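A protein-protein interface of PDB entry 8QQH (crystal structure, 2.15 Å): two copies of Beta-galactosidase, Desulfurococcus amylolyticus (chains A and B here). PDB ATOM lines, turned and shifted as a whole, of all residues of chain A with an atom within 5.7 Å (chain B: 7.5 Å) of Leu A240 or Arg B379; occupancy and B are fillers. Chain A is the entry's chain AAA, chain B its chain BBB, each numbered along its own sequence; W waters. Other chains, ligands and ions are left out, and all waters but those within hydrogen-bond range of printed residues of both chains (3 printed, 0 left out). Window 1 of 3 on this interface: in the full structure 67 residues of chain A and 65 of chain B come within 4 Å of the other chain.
The side-chain carboxylate (OD2) of Asp B354 is in hydrogen-bond range of the side-chain hydroxyl (OG) of Ser A194, at 2.9 Å.
OD2 of Asp B354 lies within salt-bridge range of NH1 of Arg A239 (3.5 Å).
N of Tyr A234 sits at hydrogen-bond distance from OD1 of Asn A238.
The side-chain amide nitrogen (ND2) of Asn B351 lies within hydrogen-bond range of the backbone carbonyl oxygen (O) of Asn B355 (2.8 Å).
The backbone carbonyl oxygen of Asn B351 sits at hydrogen-bond distance from the backbone NH of Arg B379.
The guanidinium group (NH1) of Arg B379 lies within hydrogen-bond range of the backbone carbonyl oxygen (O) of Thr B352 (3.4 Å).
The backbone NH (N) of Arg B379 is in hydrogen-bond range of the backbone carbonyl oxygen (O) of Gly B353 (2.9 Å).
The side-chain carboxylate of Asp B354 sits close to the side-chain amide oxygen of Asn B355 (3.0 Å).
Hydrophobic or aromatic side chains of chain B that line the printed part of chain A: Trp B196, Leu B356, Pro B377 and Pro B378.
Along chain A the printed residues that touch a printed residue of chain B span positions 194 to 240.
Water W3 bridges O of Asn A238 (2.6 Å) and N of Leu B356 (3.0 Å).
Water W1 lies within hydrogen-bond range of O of Arg A239, O of Ser A241 and NH2 of Arg B379.
Water W2 bridges the backbone NH (N) of Ser A241 and the side-chain carboxylate (OE2) of Glu B245.
Among the printed residues, merely in contact across the chains: Tyr A234 with Pro B377 (3.2 Å), Leu A240 with Pro B378 (3.6 Å), Pro A195 with Arg B379 (3.6 Å), Tyr A234 with Pro B378 (3.6 Å), Leu A240 with Arg B379 (3.7 Å), Asn A238 with Pro B378 (3.8 Å), Arg A239 with Asn B355 (3.8 Å), Pro A195 with Trp B196 (3.9 Å), Tyr A234 with Leu B356 (3.9 Å) and Asn A238 with Asp B354 (3.98 Å).
No position is printed for both chains.
Of the printed residues of chain B, Ser A194 touches Asp B354.
Printed residues of chain B within 4 Å of Pro A195: Trp B196 (3.9 Å) and Arg B379 (3.6 Å).
Of the printed residues of chain B, Arg A239 touches Asp B354 (3.2 Å) and Asn B355 (3.8 Å).
Leu A240 touches just these residues of chain B: Pro B378 (3.6 Å) and Arg B379 (3.7 Å).
Of the printed residues of chain A, Trp B196 touches Pro A195.
Thr B352 touches none of the printed residues of chain A.
Of the printed residues of chain A, Asp B354 touches Ser A194 (2.9 Å), Asn A238 (3.98 Å) and Arg A239 (3.2 Å).
Val B376 touches none of the printed residues of chain A.
Of chain A, only Pro A195 (3.6 Å) and Leu A240 (3.7 Å) come within 4 Å of Arg B379.
The nearest residue of chain B that does not touch Leu A240 is Glu B245 (4.5 Å).
The nearest printed residue of chain A that does not touch Asp B354 is Pro A195 (4.3 Å).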
ATOM      1  N   SER A 194       6.171 -12.855  11.517  1.00  0.00           N
ATOM      2  CA  SER A 194       7.376 -12.825  12.377  1.00  0.00           C
ATOM      3  C   SER A 194       7.774 -14.232  12.794  1.00  0.00           C
ATOM      4  O   SER A 194       6.997 -15.025  13.305  1.00  0.00           O
ATOM      5  CB  SER A 194       7.150 -11.959  13.577  1.00  0.00           C
ATOM      6  OG  SER A 194       6.611 -10.712  13.186  1.00  0.00           O
ATOM      7  N   PRO A 195       9.059 -14.570  12.654  1.00  0.00           N
ATOM      8  CA  PRO A 195       9.534 -15.903  12.967  1.00  0.00           C
ATOM      9  C   PRO A 195       8.985 -16.492  14.256  1.00  0.00           C
ATOM     10  O   PRO A 195       9.021 -15.792  15.255  1.00  0.00           O
ATOM     11  CB  PRO A 195      11.049 -15.695  13.153  1.00  0.00           C
ATOM     12  CG  PRO A 195      11.371 -14.560  12.260  1.00  0.00           C
ATOM     13  CD  PRO A 195      10.129 -13.687  12.201  1.00  0.00           C
ATOM     14  N   TYR A 234      17.837  -0.704  11.083  1.00  0.00           N
ATOM     15  CA  TYR A 234      18.854  -1.649  11.577  1.00  0.00           C
ATOM     16  C   TYR A 234      19.380  -2.403  10.375  1.00  0.00           C
ATOM     17  O   TYR A 234      18.663  -2.449   9.353  1.00  0.00           O
ATOM     18  CB  TYR A 234      18.219  -2.602  12.600  1.00  0.00           C
ATOM     19  CG  TYR A 234      17.884  -1.933  13.914  1.00  0.00           C
ATOM     20  CD1 TYR A 234      18.813  -1.839  14.934  1.00  0.00           C
ATOM     21  CD2 TYR A 234      16.642  -1.368  14.125  1.00  0.00           C
ATOM     22  CE1 TYR A 234      18.524  -1.204  16.134  1.00  0.00           C
ATOM     23  CE2 TYR A 234      16.345  -0.701  15.301  1.00  0.00           C
ATOM     24  CZ  TYR A 234      17.289  -0.615  16.311  1.00  0.00           C
ATOM     25  OH  TYR A 234      16.979   0.046  17.463  1.00  0.00           O
ATOM     26  N   TYR A 235      20.543  -3.017  10.529  1.00  0.00           N
ATOM     27  CA  TYR A 235      21.148  -3.987   9.588  1.00  0.00           C
ATOM     28  C   TYR A 235      20.849  -5.382  10.118  1.00  0.00           C
ATOM     29  O   TYR A 235      21.040  -5.609  11.305  1.00  0.00           O
ATOM     30  CB  TYR A 235      22.662  -3.762   9.476  1.00  0.00           C
ATOM     31  CG  TYR A 235      23.260  -4.568   8.358  1.00  0.00           C
ATOM     32  CD1 TYR A 235      23.237  -4.066   7.065  1.00  0.00           C
ATOM     33  CD2 TYR A 235      23.726  -5.862   8.554  1.00  0.00           C
ATOM     34  CE1 TYR A 235      23.711  -4.803   5.992  1.00  0.00           C
ATOM     35  CE2 TYR A 235      24.212  -6.615   7.486  1.00  0.00           C
ATOM     36  CZ  TYR A 235      24.199  -6.080   6.201  1.00  0.00           C
ATOM     37  OH  TYR A 235      24.656  -6.749   5.102  1.00  0.00           O
ATOM     38  N   PRO A 236      20.479  -6.383   9.291  1.00  0.00           N
ATOM     39  CA  PRO A 236      20.321  -6.219   7.845  1.00  0.00           C
ATOM     40  C   PRO A 236      18.950  -5.709   7.366  1.00  0.00           C
ATOM     41  O   PRO A 236      18.872  -5.361   6.237  1.00  0.00           O
ATOM     42  CB  PRO A 236      20.612  -7.641   7.338  1.00  0.00           C
ATOM     43  CG  PRO A 236      20.061  -8.545   8.413  1.00  0.00           C
ATOM     44  CD  PRO A 236      20.345  -7.802   9.704  1.00  0.00           C
ATOM     45  N   THR A 237      17.943  -5.659   8.248  1.00  0.00           N
ATOM     46  CA  THR A 237      16.627  -5.031   8.024  1.00  0.00           C
ATOM     47  C   THR A 237      16.167  -4.334   9.311  1.00  0.00           C
ATOM     48  O   THR A 237      16.757  -4.566  10.379  1.00  0.00           O
ATOM     49  CB  THR A 237      15.585  -6.049   7.538  1.00  0.00           C
ATOM     50  OG1 THR A 237      14.933  -6.619   8.667  1.00  0.00           O
ATOM     51  CG2 THR A 237      16.175  -7.172   6.703  1.00  0.00           C
ATOM     52  N   ASN A 238      15.140  -3.494   9.208  1.00  0.00           N
ATOM     53  CA  ASN A 238      14.494  -2.834  10.376  1.00  0.00           C
ATOM     54  C   ASN A 238      13.971  -3.907  11.361  1.00  0.00           C
ATOM     55  O   ASN A 238      13.837  -3.597  12.551  1.00  0.00           O
ATOM     56  CB  ASN A 238      13.400  -1.847   9.938  1.00  0.00           C
ATOM     57  CG  ASN A 238      13.897  -0.693   9.078  1.00  0.00           C
ATOM     58  OD1 ASN A 238      15.099  -0.436   8.932  1.00  0.00           O
ATOM     59  ND2 ASN A 238      12.975   0.050   8.503  1.00  0.00           N
ATOM     60  N   ARG A 239      13.705  -5.142  10.914  1.00  0.00           N
ATOM     61  CA  ARG A 239      13.205  -6.220  11.804  1.00  0.00           C
ATOM     62  C   ARG A 239      14.337  -7.201  12.132  1.00  0.00           C
ATOM     63  O   ARG A 239      14.021  -8.291  12.560  1.00  0.00           O
ATOM     64  CB  ARG A 239      12.082  -6.990  11.131  1.00  0.00           C
ATOM     65  CG  ARG A 239      10.845  -6.183  10.785  1.00  0.00           C
ATOM     66  CD  ARG A 239       9.846  -7.239  10.380  1.00  0.00           C
ATOM     67  NE  ARG A 239       8.564  -6.721  10.008  1.00  0.00           N
ATOM     68  CZ  ARG A 239       7.487  -7.470   9.785  1.00  0.00           C
ATOM     69  NH1 ARG A 239       7.523  -8.781   9.977  1.00  0.00           N
ATOM     70  NH2 ARG A 239       6.361  -6.881   9.423  1.00  0.00           N
ATOM     71  N   LEU A 240      15.592  -6.810  11.917  1.00  0.00           N
ATOM     72  CA  LEU A 240      16.795  -7.654  12.057  1.00  0.00           C
ATOM     73  C   LEU A 240      16.733  -8.782  11.015  1.00  0.00           C
ATOM     74  O   LEU A 240      16.142  -8.594   9.949  1.00  0.00           O
ATOM     75  CB  LEU A 240      16.910  -8.151  13.509  1.00  0.00           C
ATOM     76  CG  LEU A 240      16.832  -7.046  14.561  1.00  0.00           C
ATOM     77  CD1 LEU A 240      17.052  -7.590  15.945  1.00  0.00           C
ATOM     78  CD2 LEU A 240      17.833  -5.911  14.267  1.00  0.00           C
ATOM     79  N   SER A 241      17.407  -9.888  11.267  1.00  0.00           N
ATOM     80  CA  SER A 241      17.544 -10.963  10.274  1.00  0.00           C
ATOM     81  C   SER A 241      16.187 -11.648  10.063  1.00  0.00           C
ATOM     82  O   SER A 241      15.463 -11.896  11.028  1.00  0.00           O
ATOM     83  CB  SER A 241      18.632 -11.908  10.688  1.00  0.00           C
ATOM     84  OG  SER A 241      18.913 -12.741   9.596  1.00  0.00           O
ATOM     85  N   ILE A 242      15.771 -11.819   8.824  1.00  0.00           N
ATOM     86  CA  ILE A 242      14.638 -12.732   8.478  1.00  0.00           C
ATOM     87  C   ILE A 242      15.301 -14.071   8.177  1.00  0.00           C
ATOM     88  O   ILE A 242      15.996 -14.218   7.169  1.00  0.00           O
ATOM     89  CB  ILE A 242      13.820 -12.166   7.299  1.00  0.00           C
ATOM     90  CG1 ILE A 242      13.417 -10.702   7.529  1.00  0.00           C
ATOM     91  CG2 ILE A 242      12.594 -13.031   7.013  1.00  0.00           C
ATOM     92  CD1 ILE A 242      12.424 -10.517   8.662  1.00  0.00           C
ATOM     93  N   GLU A 288      17.725  -7.969   2.361  1.00  0.00           N
ATOM     94  CA  GLU A 288      18.225  -9.327   2.730  1.00  0.00           C
ATOM     95  C   GLU A 288      17.602 -10.371   1.774  1.00  0.00           C
ATOM     96  O   GLU A 288      17.291 -11.482   2.212  1.00  0.00           O
ATOM     97  CB  GLU A 288      17.854  -9.657   4.188  1.00  0.00           C
ATOM     98  CG  GLU A 288      18.911 -10.484   4.897  1.00  0.00           C
ATOM     99  CD  GLU A 288      18.454 -11.125   6.215  1.00  0.00           C
ATOM    100  OE1 GLU A 288      17.277 -11.005   6.560  1.00  0.00           O
ATOM    101  OE2 GLU A 288      19.296 -11.673   6.926  1.00  0.00           O
ATOM    102  N   TRP B 196      12.182 -17.661  21.424  1.00  0.00           N
ATOM    103  CA  TRP B 196      11.501 -16.339  21.238  1.00  0.00           C
ATOM    104  C   TRP B 196      10.403 -16.246  22.296  1.00  0.00           C
ATOM    105  O   TRP B 196      10.204 -15.112  22.853  1.00  0.00           O
ATOM    106  CB  TRP B 196      11.020 -15.887  19.846  1.00  0.00           C
ATOM    107  CG  TRP B 196      12.113 -15.518  18.892  1.00  0.00           C
ATOM    108  CD1 TRP B 196      12.155 -15.851  17.569  1.00  0.00           C
ATOM    109  CD2 TRP B 196      13.361 -14.857  19.180  1.00  0.00           C
ATOM    110  NE1 TRP B 196      13.328 -15.439  17.011  1.00  0.00           N
ATOM    111  CE2 TRP B 196      14.099 -14.852  17.980  1.00  0.00           C
ATOM    112  CE3 TRP B 196      13.901 -14.238  20.306  1.00  0.00           C
ATOM    113  CZ2 TRP B 196      15.360 -14.278  17.885  1.00  0.00           C
ATOM    114  CZ3 TRP B 196      15.144 -13.669  20.216  1.00  0.00           C
ATOM    115  CH2 TRP B 196      15.865 -13.703  19.028  1.00  0.00           C
ATOM    116  N   PRO B 243      20.514 -17.645  18.581  1.00  0.00           N
ATOM    117  CA  PRO B 243      20.763 -16.241  18.255  1.00  0.00           C
ATOM    118  C   PRO B 243      21.391 -15.472  19.424  1.00  0.00           C
ATOM    119  O   PRO B 243      20.993 -15.598  20.570  1.00  0.00           O
ATOM    120  CB  PRO B 243      19.394 -15.644  17.877  1.00  0.00           C
ATOM    121  CG  PRO B 243      18.486 -16.890  17.647  1.00  0.00           C
ATOM    122  CD  PRO B 243      19.074 -17.986  18.527  1.00  0.00           C
ATOM    123  N   PRO B 244      22.428 -14.670  19.160  1.00  0.00           N
ATOM    124  CA  PRO B 244      23.061 -13.890  20.213  1.00  0.00           C
ATOM    125  C   PRO B 244      22.074 -12.921  20.892  1.00  0.00           C
ATOM    126  O   PRO B 244      22.280 -12.665  22.056  1.00  0.00           O
ATOM    127  CB  PRO B 244      24.179 -13.100  19.521  1.00  0.00           C
ATOM    128  CG  PRO B 244      24.090 -13.427  18.036  1.00  0.00           C
ATOM    129  CD  PRO B 244      23.058 -14.516  17.843  1.00  0.00           C
ATOM    130  N   GLU B 245      21.071 -12.419  20.153  1.00  0.00           N
ATOM    131  CA  GLU B 245      19.950 -11.567  20.638  1.00  0.00           C
ATOM    132  C   GLU B 245      19.250 -12.318  21.777  1.00  0.00           C
ATOM    133  O   GLU B 245      18.875 -11.702  22.769  1.00  0.00           O
ATOM    134  CB  GLU B 245      18.913 -11.294  19.536  1.00  0.00           C
ATOM    135  CG  GLU B 245      19.450 -10.455  18.402  1.00  0.00           C
ATOM    136  CD  GLU B 245      20.123 -11.220  17.263  1.00  0.00           C
ATOM    137  OE1 GLU B 245      20.270 -12.430  17.395  1.00  0.00           O
ATOM    138  OE2 GLU B 245      20.525 -10.571  16.258  1.00  0.00           O
ATOM    139  N   TRP B 246      19.065 -13.603  21.590  1.00  0.00           N
ATOM    140  CA  TRP B 246      18.377 -14.493  22.549  1.00  0.00           C
ATOM    141  C   TRP B 246      19.151 -14.542  23.867  1.00  0.00           C
ATOM    142  O   TRP B 246      18.540 -14.315  24.932  1.00  0.00           O
ATOM    143  CB  TRP B 246      18.214 -15.865  21.906  1.00  0.00           C
ATOM    144  CG  TRP B 246      17.451 -16.846  22.738  1.00  0.00           C
ATOM    145  CD1 TRP B 246      17.854 -18.089  23.104  1.00  0.00           C
ATOM    146  CD2 TRP B 246      16.134 -16.671  23.298  1.00  0.00           C
ATOM    147  NE1 TRP B 246      16.879 -18.714  23.836  1.00  0.00           N
ATOM    148  CE2 TRP B 246      15.802 -17.878  23.949  1.00  0.00           C
ATOM    149  CE3 TRP B 246      15.207 -15.625  23.301  1.00  0.00           C
ATOM    150  CZ2 TRP B 246      14.603 -18.050  24.623  1.00  0.00           C
ATOM    151  CZ3 TRP B 246      14.018 -15.793  23.974  1.00  0.00           C
ATOM    152  CH2 TRP B 246      13.721 -16.998  24.611  1.00  0.00           C
ATOM    153  N   GLU B 248      21.366 -12.449  25.084  1.00  0.00           N
ATOM    154  CA  GLU B 248      21.288 -11.149  25.804  1.00  0.00           C
ATOM    155  C   GLU B 248      19.911 -10.986  26.485  1.00  0.00           C
ATOM    156  O   GLU B 248      19.883 -10.541  27.634  1.00  0.00           O
ATOM    157  CB  GLU B 248      21.601  -9.975  24.893  1.00  0.00           C
ATOM    158  CG  GLU B 248      21.740  -8.686  25.668  1.00  0.00           C
ATOM    159  CD  GLU B 248      22.042  -7.450  24.838  1.00  0.00           C
ATOM    160  OE1 GLU B 248      22.388  -7.598  23.664  1.00  0.00           O
ATOM    161  OE2 GLU B 248      21.923  -6.330  25.390  1.00  0.00           O
ATOM    162  N   ILE B 249      18.807 -11.336  25.821  1.00  0.00           N
ATOM    163  CA  ILE B 249      17.449 -11.264  26.421  1.00  0.00           C
ATOM    164  C   ILE B 249      17.376 -12.161  27.678  1.00  0.00           C
ATOM    165  O   ILE B 249      16.752 -11.712  28.678  1.00  0.00           O
ATOM    166  CB  ILE B 249      16.378 -11.632  25.367  1.00  0.00           C
ATOM    167  CG1 ILE B 249      16.060 -10.454  24.449  1.00  0.00           C
ATOM    168  CG2 ILE B 249      15.094 -12.176  25.994  1.00  0.00           C
ATOM    169  CD1 ILE B 249      15.280 -10.903  23.221  1.00  0.00           C
ATOM    170  N   ARG B 303      27.770  -8.975  23.208  1.00  0.00           N
ATOM    171  CA  ARG B 303      26.486  -8.716  23.914  1.00  0.00           C
ATOM    172  C   ARG B 303      26.634  -9.065  25.384  1.00  0.00           C
ATOM    173  O   ARG B 303      26.228  -8.254  26.248  1.00  0.00           O
ATOM    174  CB  ARG B 303      25.350  -9.511  23.294  1.00  0.00           C
ATOM    175  CG  ARG B 303      25.054  -9.069  21.874  1.00  0.00           C
ATOM    176  CD  ARG B 303      23.808  -9.774  21.451  1.00  0.00           C
ATOM    177  NE  ARG B 303      23.355  -9.217  20.213  1.00  0.00           N
ATOM    178  CZ  ARG B 303      22.280  -8.475  19.992  1.00  0.00           C
ATOM    179  NH1 ARG B 303      21.427  -8.121  20.948  1.00  0.00           N
ATOM    180  NH2 ARG B 303      22.061  -8.114  18.745  1.00  0.00           N
ATOM    181  N   ARG B 350      11.615  -5.121  27.984  1.00  0.00           N
ATOM    182  CA  ARG B 350      11.887  -6.336  27.182  1.00  0.00           C
ATOM    183  C   ARG B 350      10.974  -6.325  25.953  1.00  0.00           C
ATOM    184  O   ARG B 350       9.771  -6.199  26.079  1.00  0.00           O
ATOM    185  CB  ARG B 350      11.785  -7.583  28.055  1.00  0.00           C
ATOM    186  CG  ARG B 350      11.962  -8.886  27.282  1.00  0.00           C
ATOM    187  CD  ARG B 350      10.845  -9.843  27.682  1.00  0.00           C
ATOM    188  NE  ARG B 350      11.364 -10.642  28.702  1.00  0.00           N
ATOM    189  CZ  ARG B 350      10.710 -11.440  29.522  1.00  0.00           C
ATOM    190  NH1 ARG B 350       9.405 -11.603  29.502  1.00  0.00           N
ATOM    191  NH2 ARG B 350      11.451 -12.126  30.359  1.00  0.00           N
ATOM    192  N   ASN B 351      11.577  -6.373  24.779  1.00  0.00           N
ATOM    193  CA  ASN B 351      10.853  -6.404  23.489  1.00  0.00           C
ATOM    194  C   ASN B 351      11.331  -7.639  22.731  1.00  0.00           C
ATOM    195  O   ASN B 351      12.358  -7.528  22.011  1.00  0.00           O
ATOM    196  CB  ASN B 351      11.089  -5.095  22.732  1.00  0.00           C
ATOM    197  CG  ASN B 351      10.387  -5.055  21.393  1.00  0.00           C
ATOM    198  OD1 ASN B 351       9.571  -5.925  21.113  1.00  0.00           O
ATOM    199  ND2 ASN B 351      10.774  -4.108  20.551  1.00  0.00           N
ATOM    200  N   THR B 352      10.621  -8.755  22.908  1.00  0.00           N
ATOM    201  CA  THR B 352      10.872 -10.047  22.228  1.00  0.00           C
ATOM    202  C   THR B 352      10.353 -10.027  20.773  1.00  0.00           C
ATOM    203  O   THR B 352      10.642 -10.974  20.098  1.00  0.00           O
ATOM    204  CB  THR B 352      10.185 -11.197  22.963  1.00  0.00           C
ATOM    205  OG1 THR B 352       8.824 -10.797  23.070  1.00  0.00           O
ATOM    206  CG2 THR B 352      10.778 -11.487  24.322  1.00  0.00           C
ATOM    207  N   GLY B 353       9.615  -9.004  20.351  1.00  0.00           N
ATOM    208  CA  GLY B 353       9.064  -8.861  18.989  1.00  0.00           C
ATOM    209  C   GLY B 353      10.073  -8.224  18.045  1.00  0.00           C
ATOM    210  O   GLY B 353      11.215  -7.908  18.478  1.00  0.00           O
ATOM    211  N   ASP B 354       9.719  -8.107  16.770  1.00  0.00           N
ATOM    212  CA  ASP B 354      10.718  -7.787  15.728  1.00  0.00           C
ATOM    213  C   ASP B 354      10.526  -6.340  15.262  1.00  0.00           C
ATOM    214  O   ASP B 354      11.149  -5.967  14.282  1.00  0.00           O
ATOM    215  CB  ASP B 354      10.668  -8.832  14.612  1.00  0.00           C
ATOM    216  CG  ASP B 354       9.333  -8.813  13.879  1.00  0.00           C
ATOM    217  OD1 ASP B 354       8.437  -8.041  14.300  1.00  0.00           O
ATOM    218  OD2 ASP B 354       9.216  -9.534  12.905  1.00  0.00           O
ATOM    219  N   ASN B 355       9.695  -5.554  15.937  1.00  0.00           N
ATOM    220  CA  ASN B 355       9.491  -4.126  15.600  1.00  0.00           C
ATOM    221  C   ASN B 355      10.017  -3.292  16.784  1.00  0.00           C
ATOM    222  O   ASN B 355       9.829  -3.659  17.928  1.00  0.00           O
ATOM    223  CB  ASN B 355       8.047  -3.818  15.150  1.00  0.00           C
ATOM    224  CG  ASN B 355       7.637  -4.530  13.857  1.00  0.00           C
ATOM    225  OD1 ASN B 355       6.896  -5.510  13.887  1.00  0.00           O
ATOM    226  ND2 ASN B 355       8.119  -4.087  12.702  1.00  0.00           N
ATOM    227  N   LEU B 356      10.699  -2.202  16.476  1.00  0.00           N
ATOM    228  CA  LEU B 356      11.150  -1.178  17.438  1.00  0.00           C
ATOM    229  C   LEU B 356       9.919  -0.665  18.194  1.00  0.00           C
ATOM    230  O   LEU B 356       8.893  -0.483  17.572  1.00  0.00           O
ATOM    231  CB  LEU B 356      11.847  -0.081  16.636  1.00  0.00           C
ATOM    232  CG  LEU B 356      12.278   1.146  17.420  1.00  0.00           C
ATOM    233  CD1 LEU B 356      13.531   1.766  16.830  1.00  0.00           C
ATOM    234  CD2 LEU B 356      11.150   2.147  17.424  1.00  0.00           C
ATOM    235  N   VAL B 376      13.010   1.023  22.558  1.00  0.00           N
ATOM    236  CA  VAL B 376      13.291  -0.397  22.895  1.00  0.00           C
ATOM    237  C   VAL B 376      13.481  -1.114  21.567  1.00  0.00           C
ATOM    238  O   VAL B 376      12.515  -1.328  20.830  1.00  0.00           O
ATOM    239  CB  VAL B 376      12.209  -1.050  23.777  1.00  0.00           C
ATOM    240  CG1 VAL B 376      12.748  -2.329  24.379  1.00  0.00           C
ATOM    241  CG2 VAL B 376      11.732  -0.123  24.881  1.00  0.00           C
ATOM    242  N   PRO B 377      14.743  -1.388  21.177  1.00  0.00           N
ATOM    243  CA  PRO B 377      15.021  -2.014  19.879  1.00  0.00           C
ATOM    244  C   PRO B 377      14.334  -3.371  19.743  1.00  0.00           C
ATOM    245  O   PRO B 377      13.940  -3.972  20.741  1.00  0.00           O
ATOM    246  CB  PRO B 377      16.552  -2.148  19.806  1.00  0.00           C
ATOM    247  CG  PRO B 377      17.068  -1.160  20.877  1.00  0.00           C
ATOM    248  CD  PRO B 377      15.973  -1.046  21.919  1.00  0.00           C
ATOM    249  N   PRO B 378      14.138  -3.850  18.496  1.00  0.00           N
ATOM    250  CA  PRO B 378      13.611  -5.195  18.243  1.00  0.00           C
ATOM    251  C   PRO B 378      14.528  -6.277  18.843  1.00  0.00           C
ATOM    252  O   PRO B 378      15.754  -6.057  18.891  1.00  0.00           O
ATOM    253  CB  PRO B 378      13.580  -5.334  16.714  1.00  0.00           C
ATOM    254  CG  PRO B 378      14.442  -4.217  16.202  1.00  0.00           C
ATOM    255  CD  PRO B 378      14.559  -3.162  17.273  1.00  0.00           C
ATOM    256  N   ARG B 379      13.930  -7.344  19.379  1.00  0.00           N
ATOM    257  CA  ARG B 379      14.652  -8.492  19.980  1.00  0.00           C
ATOM    258  C   ARG B 379      15.703  -7.998  20.977  1.00  0.00           C
ATOM    259  O   ARG B 379      16.908  -8.398  20.860  1.00  0.00           O
ATOM    260  CB  ARG B 379      15.363  -9.292  18.890  1.00  0.00           C
ATOM    261  CG  ARG B 379      14.460  -9.615  17.715  1.00  0.00           C
ATOM    262  CD  ARG B 379      14.109 -11.050  17.740  1.00  0.00           C
ATOM    263  NE  ARG B 379      13.736 -11.433  16.395  1.00  0.00           N
ATOM    264  CZ  ARG B 379      12.561 -11.910  16.071  1.00  0.00           C
ATOM    265  NH1 ARG B 379      11.640 -12.072  17.014  1.00  0.00           N
ATOM    266  NH2 ARG B 379      12.326 -12.209  14.803  1.00  0.00           N
ATOM    267  N   TYR B 380      15.267  -7.176  21.917  1.00  0.00           N
ATOM    268  CA  TYR B 380      16.162  -6.504  22.885  1.00  0.00           C
ATOM    269  C   TYR B 380      15.415  -6.294  24.192  1.00  0.00           C
ATOM    270  O   TYR B 380      14.155  -6.089  24.219  1.00  0.00           O
ATOM    271  CB  TYR B 380      16.638  -5.210  22.230  1.00  0.00           C
ATOM    272  CG  TYR B 380      17.878  -4.633  22.839  1.00  0.00           C
ATOM    273  CD1 TYR B 380      19.128  -5.056  22.423  1.00  0.00           C
ATOM    274  CD2 TYR B 380      17.804  -3.670  23.835  1.00  0.00           C
ATOM    275  CE1 TYR B 380      20.282  -4.533  22.992  1.00  0.00           C
ATOM    276  CE2 TYR B 380      18.947  -3.151  24.412  1.00  0.00           C
ATOM    277  CZ  TYR B 380      20.192  -3.563  23.973  1.00  0.00           C
ATOM    278  OH  TYR B 380      21.322  -3.060  24.532  1.00  0.00           O
ATOM    279  N   ALA B 381      16.191  -6.325  25.264  1.00  0.00           N
ATOM    280  CA  ALA B 381      15.785  -5.862  26.602  1.00  0.00           C
ATOM    281  C   ALA B 381      16.777  -4.788  27.078  1.00  0.00           C
ATOM    282  O   ALA B 381      17.966  -5.045  27.098  1.00  0.00           O
ATOM    283  CB  ALA B 381      15.703  -7.039  27.515  1.00  0.00           C
ATOM    284  N   ARG B 484      26.163   1.603  20.595  1.00  0.00           N
ATOM    285  CA  ARG B 484      26.226   0.199  21.049  1.00  0.00           C
ATOM    286  C   ARG B 484      27.510  -0.497  20.563  1.00  0.00           C
ATOM    287  O   ARG B 484      28.128  -1.224  21.372  1.00  0.00           O
ATOM    288  CB  ARG B 484      24.968  -0.528  20.561  1.00  0.00           C
ATOM    289  CG  ARG B 484      24.714  -1.811  21.335  1.00  0.00           C
ATOM    290  CD  ARG B 484      23.921  -2.806  20.514  1.00  0.00           C
ATOM    291  NE  ARG B 484      22.563  -2.352  20.261  1.00  0.00           N
ATOM    292  CZ  ARG B 484      21.612  -3.107  19.716  1.00  0.00           C
ATOM    293  NH1 ARG B 484      21.855  -4.379  19.446  1.00  0.00           N
ATOM    294  NH2 ARG B 484      20.395  -2.611  19.512  1.00  0.00           N
HETATM  295  O   HOH W   1      13.099 -10.789  12.256  1.00  0.00           O
HETATM  296  O   HOH W   2      19.098 -10.913  13.553  1.00  0.00           O
HETATM  297  O   HOH W   3      11.955  -2.170  13.746  1.00  0.00           O
